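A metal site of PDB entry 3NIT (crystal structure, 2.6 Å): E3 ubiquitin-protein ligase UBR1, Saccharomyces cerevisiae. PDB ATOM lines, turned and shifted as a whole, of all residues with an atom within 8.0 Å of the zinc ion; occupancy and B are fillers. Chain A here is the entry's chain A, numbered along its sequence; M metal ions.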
ATOM      1  N   ARG A  31     -14.935  22.026 -19.792  1.00  0.00           N
ATOM      2  CA  ARG A  31     -14.425  22.749 -20.952  1.00  0.00           C
ATOM      3  C   ARG A  31     -13.072  23.316 -20.574  1.00  0.00           C
ATOM      4  O   ARG A  31     -12.891  23.749 -19.434  1.00  0.00           O
ATOM      5  CB  ARG A  31     -15.376  23.888 -21.333  1.00  0.00           C
ATOM      6  CG  ARG A  31     -16.645  23.437 -22.042  1.00  0.00           C
ATOM      7  CD  ARG A  31     -17.432  24.602 -22.608  1.00  0.00           C
ATOM      8  NE  ARG A  31     -18.221  25.294 -21.596  1.00  0.00           N
ATOM      9  CZ  ARG A  31     -18.939  26.397 -21.800  1.00  0.00           C
ATOM     10  NH1 ARG A  31     -18.979  26.959 -23.013  1.00  0.00           N
ATOM     11  NH2 ARG A  31     -19.619  26.951 -20.809  1.00  0.00           N
ATOM     12  N   CYS A  32     -12.132  23.323 -21.515  1.00  0.00           N
ATOM     13  CA  CYS A  32     -10.810  23.910 -21.306  1.00  0.00           C
ATOM     14  C   CYS A  32     -10.532  25.020 -22.314  1.00  0.00           C
ATOM     15  O   CYS A  32     -10.621  24.794 -23.524  1.00  0.00           O
ATOM     16  CB  CYS A  32      -9.718  22.843 -21.387  1.00  0.00           C
ATOM     17  SG  CYS A  32      -8.032  23.490 -21.289  1.00  0.00           S
ATOM     18  N   HIS A  33     -10.179  26.195 -21.817  1.00  0.00           N
ATOM     19  CA  HIS A  33      -9.944  27.360 -22.682  1.00  0.00           C
ATOM     20  C   HIS A  33      -8.783  27.155 -23.655  1.00  0.00           C
ATOM     21  O   HIS A  33      -8.855  27.577 -24.811  1.00  0.00           O
ATOM     22  CB  HIS A  33      -9.733  28.621 -21.842  1.00  0.00           C
ATOM     23  CG  HIS A  33      -9.310  29.814 -22.636  1.00  0.00           C
ATOM     24  ND1 HIS A  33     -10.205  30.676 -23.228  1.00  0.00           N
ATOM     25  CD2 HIS A  33      -8.080  30.286 -22.934  1.00  0.00           C
ATOM     26  CE1 HIS A  33      -9.545  31.633 -23.852  1.00  0.00           C
ATOM     27  NE2 HIS A  33      -8.250  31.420 -23.690  1.00  0.00           N
ATOM     28  N   GLU A  34      -7.713  26.508 -23.193  1.00  0.00           N
ATOM     29  CA  GLU A  34      -6.538  26.267 -24.017  1.00  0.00           C
ATOM     30  C   GLU A  34      -6.773  25.159 -25.047  1.00  0.00           C
ATOM     31  O   GLU A  34      -6.381  25.296 -26.211  1.00  0.00           O
ATOM     32  CB  GLU A  34      -5.327  25.926 -23.141  1.00  0.00           C
ATOM     33  CG  GLU A  34      -4.668  27.123 -22.431  1.00  0.00           C
ATOM     34  CD  GLU A  34      -5.466  27.707 -21.255  1.00  0.00           C
ATOM     35  OE1 GLU A  34      -5.163  28.845 -20.852  1.00  0.00           O
ATOM     36  OE2 GLU A  34      -6.393  27.041 -20.726  1.00  0.00           O
ATOM     37  N   CYS A  35      -7.407  24.066 -24.634  1.00  0.00           N
ATOM     38  CA  CYS A  35      -7.539  22.860 -25.475  1.00  0.00           C
ATOM     39  C   CYS A  35      -8.695  22.857 -26.476  1.00  0.00           C
ATOM     40  O   CYS A  35      -8.562  22.299 -27.563  1.00  0.00           O
ATOM     41  CB  CYS A  35      -7.622  21.606 -24.616  1.00  0.00           C
ATOM     42  SG  CYS A  35      -6.224  21.378 -23.523  1.00  0.00           S
ATOM     43  N   GLY A  36      -9.834  23.452 -26.116  1.00  0.00           N
ATOM     44  CA  GLY A  36     -11.030  23.417 -26.960  1.00  0.00           C
ATOM     45  C   GLY A  36     -11.024  24.413 -28.104  1.00  0.00           C
ATOM     46  O   GLY A  36     -10.590  25.549 -27.919  1.00  0.00           O
ATOM     47  N   LEU A  43     -16.150  17.855 -22.368  1.00  0.00           N
ATOM     48  CA  LEU A  43     -15.769  16.531 -21.885  1.00  0.00           C
ATOM     49  C   LEU A  43     -16.674  16.076 -20.744  1.00  0.00           C
ATOM     50  O   LEU A  43     -17.095  16.873 -19.907  1.00  0.00           O
ATOM     51  CB  LEU A  43     -14.308  16.546 -21.432  1.00  0.00           C
ATOM     52  CG  LEU A  43     -13.231  16.848 -22.474  1.00  0.00           C
ATOM     53  CD1 LEU A  43     -11.913  17.154 -21.797  1.00  0.00           C
ATOM     54  CD2 LEU A  43     -13.080  15.700 -23.431  1.00  0.00           C
ATOM     55  N   PHE A  48     -12.828  13.390 -18.893  1.00  0.00           N
ATOM     56  CA  PHE A  48     -11.999  14.497 -18.450  1.00  0.00           C
ATOM     57  C   PHE A  48     -10.862  14.019 -17.576  1.00  0.00           C
ATOM     58  O   PHE A  48     -11.094  13.364 -16.559  1.00  0.00           O
ATOM     59  CB  PHE A  48     -12.826  15.549 -17.707  1.00  0.00           C
ATOM     60  CG  PHE A  48     -12.017  16.700 -17.172  1.00  0.00           C
ATOM     61  CD1 PHE A  48     -11.509  17.683 -18.021  1.00  0.00           C
ATOM     62  CD2 PHE A  48     -11.756  16.797 -15.806  1.00  0.00           C
ATOM     63  CE1 PHE A  48     -10.766  18.731 -17.524  1.00  0.00           C
ATOM     64  CE2 PHE A  48     -11.009  17.850 -15.301  1.00  0.00           C
ATOM     65  CZ  PHE A  48     -10.512  18.813 -16.158  1.00  0.00           C
ATOM     66  N   ASN A  49      -9.637  14.332 -17.999  1.00  0.00           N
ATOM     67  CA  ASN A  49      -8.441  13.922 -17.296  1.00  0.00           C
ATOM     68  C   ASN A  49      -7.660  15.128 -16.795  1.00  0.00           C
ATOM     69  O   ASN A  49      -7.061  15.843 -17.596  1.00  0.00           O
ATOM     70  CB  ASN A  49      -7.580  13.071 -18.230  1.00  0.00           C
ATOM     71  CG  ASN A  49      -6.431  12.365 -17.520  1.00  0.00           C
ATOM     72  OD1 ASN A  49      -6.039  12.729 -16.394  1.00  0.00           O
ATOM     73  ND2 ASN A  49      -5.871  11.359 -18.165  1.00  0.00           N
ATOM     74  N   PRO A  50      -7.628  15.356 -15.468  1.00  0.00           N
ATOM     75  CA  PRO A  50      -7.017  16.555 -14.924  1.00  0.00           C
ATOM     76  C   PRO A  50      -5.578  16.705 -15.393  1.00  0.00           C
ATOM     77  O   PRO A  50      -5.111  17.828 -15.627  1.00  0.00           O
ATOM     78  CB  PRO A  50      -7.059  16.329 -13.413  1.00  0.00           C
ATOM     79  CG  PRO A  50      -8.156  15.385 -13.206  1.00  0.00           C
ATOM     80  CD  PRO A  50      -8.139  14.477 -14.399  1.00  0.00           C
ATOM     81  N   LYS A  51      -4.883  15.567 -15.550  1.00  0.00           N
ATOM     82  CA  LYS A  51      -3.498  15.543 -16.019  1.00  0.00           C
ATOM     83  C   LYS A  51      -3.295  16.310 -17.322  1.00  0.00           C
ATOM     84  O   LYS A  51      -2.314  17.033 -17.467  1.00  0.00           O
ATOM     85  CB  LYS A  51      -3.038  14.092 -16.186  1.00  0.00           C
ATOM     86  CG  LYS A  51      -2.673  13.378 -14.884  1.00  0.00           C
ATOM     87  CD  LYS A  51      -2.656  11.860 -15.100  1.00  0.00           C
ATOM     88  CE  LYS A  51      -1.731  11.128 -14.120  1.00  0.00           C
ATOM     89  NZ  LYS A  51      -2.165  11.227 -12.688  1.00  0.00           N
ATOM     90  N   ASP A  52      -4.234  16.194 -18.253  1.00  0.00           N
ATOM     91  CA  ASP A  52      -4.128  16.883 -19.533  1.00  0.00           C
ATOM     92  C   ASP A  52      -4.211  18.399 -19.449  1.00  0.00           C
ATOM     93  O   ASP A  52      -3.907  19.093 -20.419  1.00  0.00           O
ATOM     94  CB  ASP A  52      -5.218  16.389 -20.492  1.00  0.00           C
ATOM     95  CG  ASP A  52      -4.955  14.998 -20.984  1.00  0.00           C
ATOM     96  OD1 ASP A  52      -3.766  14.635 -21.121  1.00  0.00           O
ATOM     97  OD2 ASP A  52      -5.935  14.258 -21.231  1.00  0.00           O
ATOM     98  N   HIS A  53      -4.644  18.915 -18.298  1.00  0.00           N
ATOM     99  CA  HIS A  53      -5.053  20.320 -18.209  1.00  0.00           C
ATOM    100  C   HIS A  53      -4.397  21.079 -17.073  1.00  0.00           C
ATOM    101  O   HIS A  53      -4.870  22.153 -16.682  1.00  0.00           O
ATOM    102  CB  HIS A  53      -6.576  20.418 -18.170  1.00  0.00           C
ATOM    103  CG  HIS A  53      -7.242  19.604 -19.234  1.00  0.00           C
ATOM    104  ND1 HIS A  53      -7.332  20.024 -20.540  1.00  0.00           N
ATOM    105  CD2 HIS A  53      -7.813  18.382 -19.183  1.00  0.00           C
ATOM    106  CE1 HIS A  53      -7.948  19.100 -21.255  1.00  0.00           C
ATOM    107  NE2 HIS A  53      -8.249  18.089 -20.456  1.00  0.00           N
ATOM    108  N   VAL A  54      -3.308  20.520 -16.559  1.00  0.00           N
ATOM    109  CA  VAL A  54      -2.467  21.207 -15.584  1.00  0.00           C
ATOM    110  C   VAL A  54      -2.093  22.555 -16.182  1.00  0.00           C
ATOM    111  O   VAL A  54      -1.633  22.649 -17.322  1.00  0.00           O
ATOM    112  CB  VAL A  54      -1.188  20.408 -15.221  1.00  0.00           C
ATOM    113  CG1 VAL A  54      -0.380  21.159 -14.173  1.00  0.00           C
ATOM    114  CG2 VAL A  54      -1.533  18.993 -14.728  1.00  0.00           C
ATOM    115  N   ASN A  55      -2.348  23.605 -15.408  1.00  0.00           N
ATOM    116  CA  ASN A  55      -2.026  24.979 -15.783  1.00  0.00           C
ATOM    117  C   ASN A  55      -2.985  25.579 -16.795  1.00  0.00           C
ATOM    118  O   ASN A  55      -2.807  26.723 -17.213  1.00  0.00           O
ATOM    119  CB  ASN A  55      -0.579  25.072 -16.283  1.00  0.00           C
ATOM    120  CG  ASN A  55       0.168  26.216 -15.648  1.00  0.00           C
ATOM    121  OD1 ASN A  55      -0.213  27.384 -15.785  1.00  0.00           O
ATOM    122  ND2 ASN A  55       1.243  25.892 -14.926  1.00  0.00           N
ATOM    123  N   HIS A  56      -4.008  24.819 -17.185  1.00  0.00           N
ATOM    124  CA  HIS A  56      -5.054  25.307 -18.100  1.00  0.00           C
ATOM    125  C   HIS A  56      -6.224  25.888 -17.330  1.00  0.00           C
ATOM    126  O   HIS A  56      -6.417  25.583 -16.155  1.00  0.00           O
ATOM    127  CB  HIS A  56      -5.555  24.185 -19.009  1.00  0.00           C
ATOM    128  CG  HIS A  56      -4.525  23.663 -19.968  1.00  0.00           C
ATOM    129  ND1 HIS A  56      -4.577  22.376 -20.476  1.00  0.00           N
ATOM    130  CD2 HIS A  56      -3.421  24.239 -20.499  1.00  0.00           C
ATOM    131  CE1 HIS A  56      -3.549  22.189 -21.275  1.00  0.00           C
ATOM    132  NE2 HIS A  56      -2.832  23.291 -21.311  1.00  0.00           N
ATOM    133  N   HIS A  57      -7.016  26.727 -17.997  1.00  0.00           N
ATOM    134  CA  HIS A  57      -8.238  27.293 -17.430  1.00  0.00           C
ATOM    135  C   HIS A  57      -9.419  26.381 -17.721  1.00  0.00           C
ATOM    136  O   HIS A  57     -10.050  26.474 -18.767  1.00  0.00           O
ATOM    137  CB  HIS A  57      -8.511  28.677 -17.989  1.00  0.00           C
ATOM    138  CG  HIS A  57      -7.480  29.689 -17.615  1.00  0.00           C
ATOM    139  ND1 HIS A  57      -6.274  29.784 -18.257  1.00  0.00           N
ATOM    140  CD2 HIS A  57      -7.482  30.651 -16.666  1.00  0.00           C
ATOM    141  CE1 HIS A  57      -5.561  30.757 -17.716  1.00  0.00           C
ATOM    142  NE2 HIS A  57      -6.280  31.300 -16.741  1.00  0.00           N
ATOM    143  N   VAL A  58      -9.711  25.490 -16.787  1.00  0.00           N
ATOM    144  CA  VAL A  58     -10.832  24.570 -16.937  1.00  0.00           C
ATOM    145  C   VAL A  58     -12.098  25.205 -16.382  1.00  0.00           C
ATOM    146  O   VAL A  58     -12.103  25.792 -15.299  1.00  0.00           O
ATOM    147  CB  VAL A  58     -10.558  23.197 -16.300  1.00  0.00           C
ATOM    148  CG1 VAL A  58     -11.754  22.285 -16.439  1.00  0.00           C
ATOM    149  CG2 VAL A  58      -9.359  22.567 -16.967  1.00  0.00           C
ATOM    150  N   TRP A  79     -10.291  19.439 -30.552  1.00  0.00           N
ATOM    151  CA  TRP A  79      -9.210  19.680 -29.602  1.00  0.00           C
ATOM    152  C   TRP A  79      -7.909  20.099 -30.261  1.00  0.00           C
ATOM    153  O   TRP A  79      -7.486  19.486 -31.243  1.00  0.00           O
ATOM    154  CB  TRP A  79      -8.994  18.441 -28.729  1.00  0.00           C
ATOM    155  CG  TRP A  79     -10.257  18.016 -28.068  1.00  0.00           C
ATOM    156  CD1 TRP A  79     -11.002  16.913 -28.362  1.00  0.00           C
ATOM    157  CD2 TRP A  79     -10.952  18.715 -27.022  1.00  0.00           C
ATOM    158  NE1 TRP A  79     -12.114  16.870 -27.554  1.00  0.00           N
ATOM    159  CE2 TRP A  79     -12.110  17.961 -26.720  1.00  0.00           C
ATOM    160  CE3 TRP A  79     -10.706  19.893 -26.305  1.00  0.00           C
ATOM    161  CZ2 TRP A  79     -13.020  18.358 -25.734  1.00  0.00           C
ATOM    162  CZ3 TRP A  79     -11.616  20.277 -25.323  1.00  0.00           C
ATOM    163  CH2 TRP A  79     -12.749  19.510 -25.047  1.00  0.00           C
ATOM    164  N   SER A  81      -4.975  20.021 -28.688  1.00  0.00           N
ATOM    165  CA  SER A  81      -3.954  19.118 -28.204  1.00  0.00           C
ATOM    166  C   SER A  81      -4.541  17.714 -28.102  1.00  0.00           C
ATOM    167  O   SER A  81      -5.749  17.573 -27.871  1.00  0.00           O
ATOM    168  CB  SER A  81      -3.453  19.597 -26.834  1.00  0.00           C
ATOM    169  OG  SER A  81      -2.741  18.577 -26.129  1.00  0.00           O
ATOM    170  N   LEU A  83      -5.697  14.476 -26.327  1.00  0.00           N
ATOM    171  CA  LEU A  83      -6.148  14.211 -24.969  1.00  0.00           C
ATOM    172  C   LEU A  83      -5.879  12.765 -24.580  1.00  0.00           C
ATOM    173  O   LEU A  83      -5.625  11.915 -25.433  1.00  0.00           O
ATOM    174  CB  LEU A  83      -7.627  14.540 -24.813  1.00  0.00           C
ATOM    175  CG  LEU A  83      -8.026  15.977 -25.124  1.00  0.00           C
ATOM    176  CD1 LEU A  83      -9.518  16.123 -25.002  1.00  0.00           C
ATOM    177  CD2 LEU A  83      -7.310  16.976 -24.223  1.00  0.00           C
HETATM  178 ZN    ZN M   1      -6.561  21.765 -21.456  1.00  0.00          ZN
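The zinc ion is bound by ND1 of His 53 (2.1 Å), SG of Cys 35 (2.1 Å), SG of Cys 32 (2.3 Å) and ND1 of His 56 (2.3 Å).
The zinc ion has four donor atoms within binding distance.
N of Glu 34 sits close to SG of Cys 32.
The backbone carbonyl oxygen (O) of Asp 52 sits close to a ring nitrogen (ND1) of His 56 (3.4 Å).
Residues that only touch the zinc ion: Asp 52 (3.9 Å).
Five residues have an atom within 4 Å of the zinc ion: Cys 32, Cys 35, Asp 52, His 53 and His 56.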
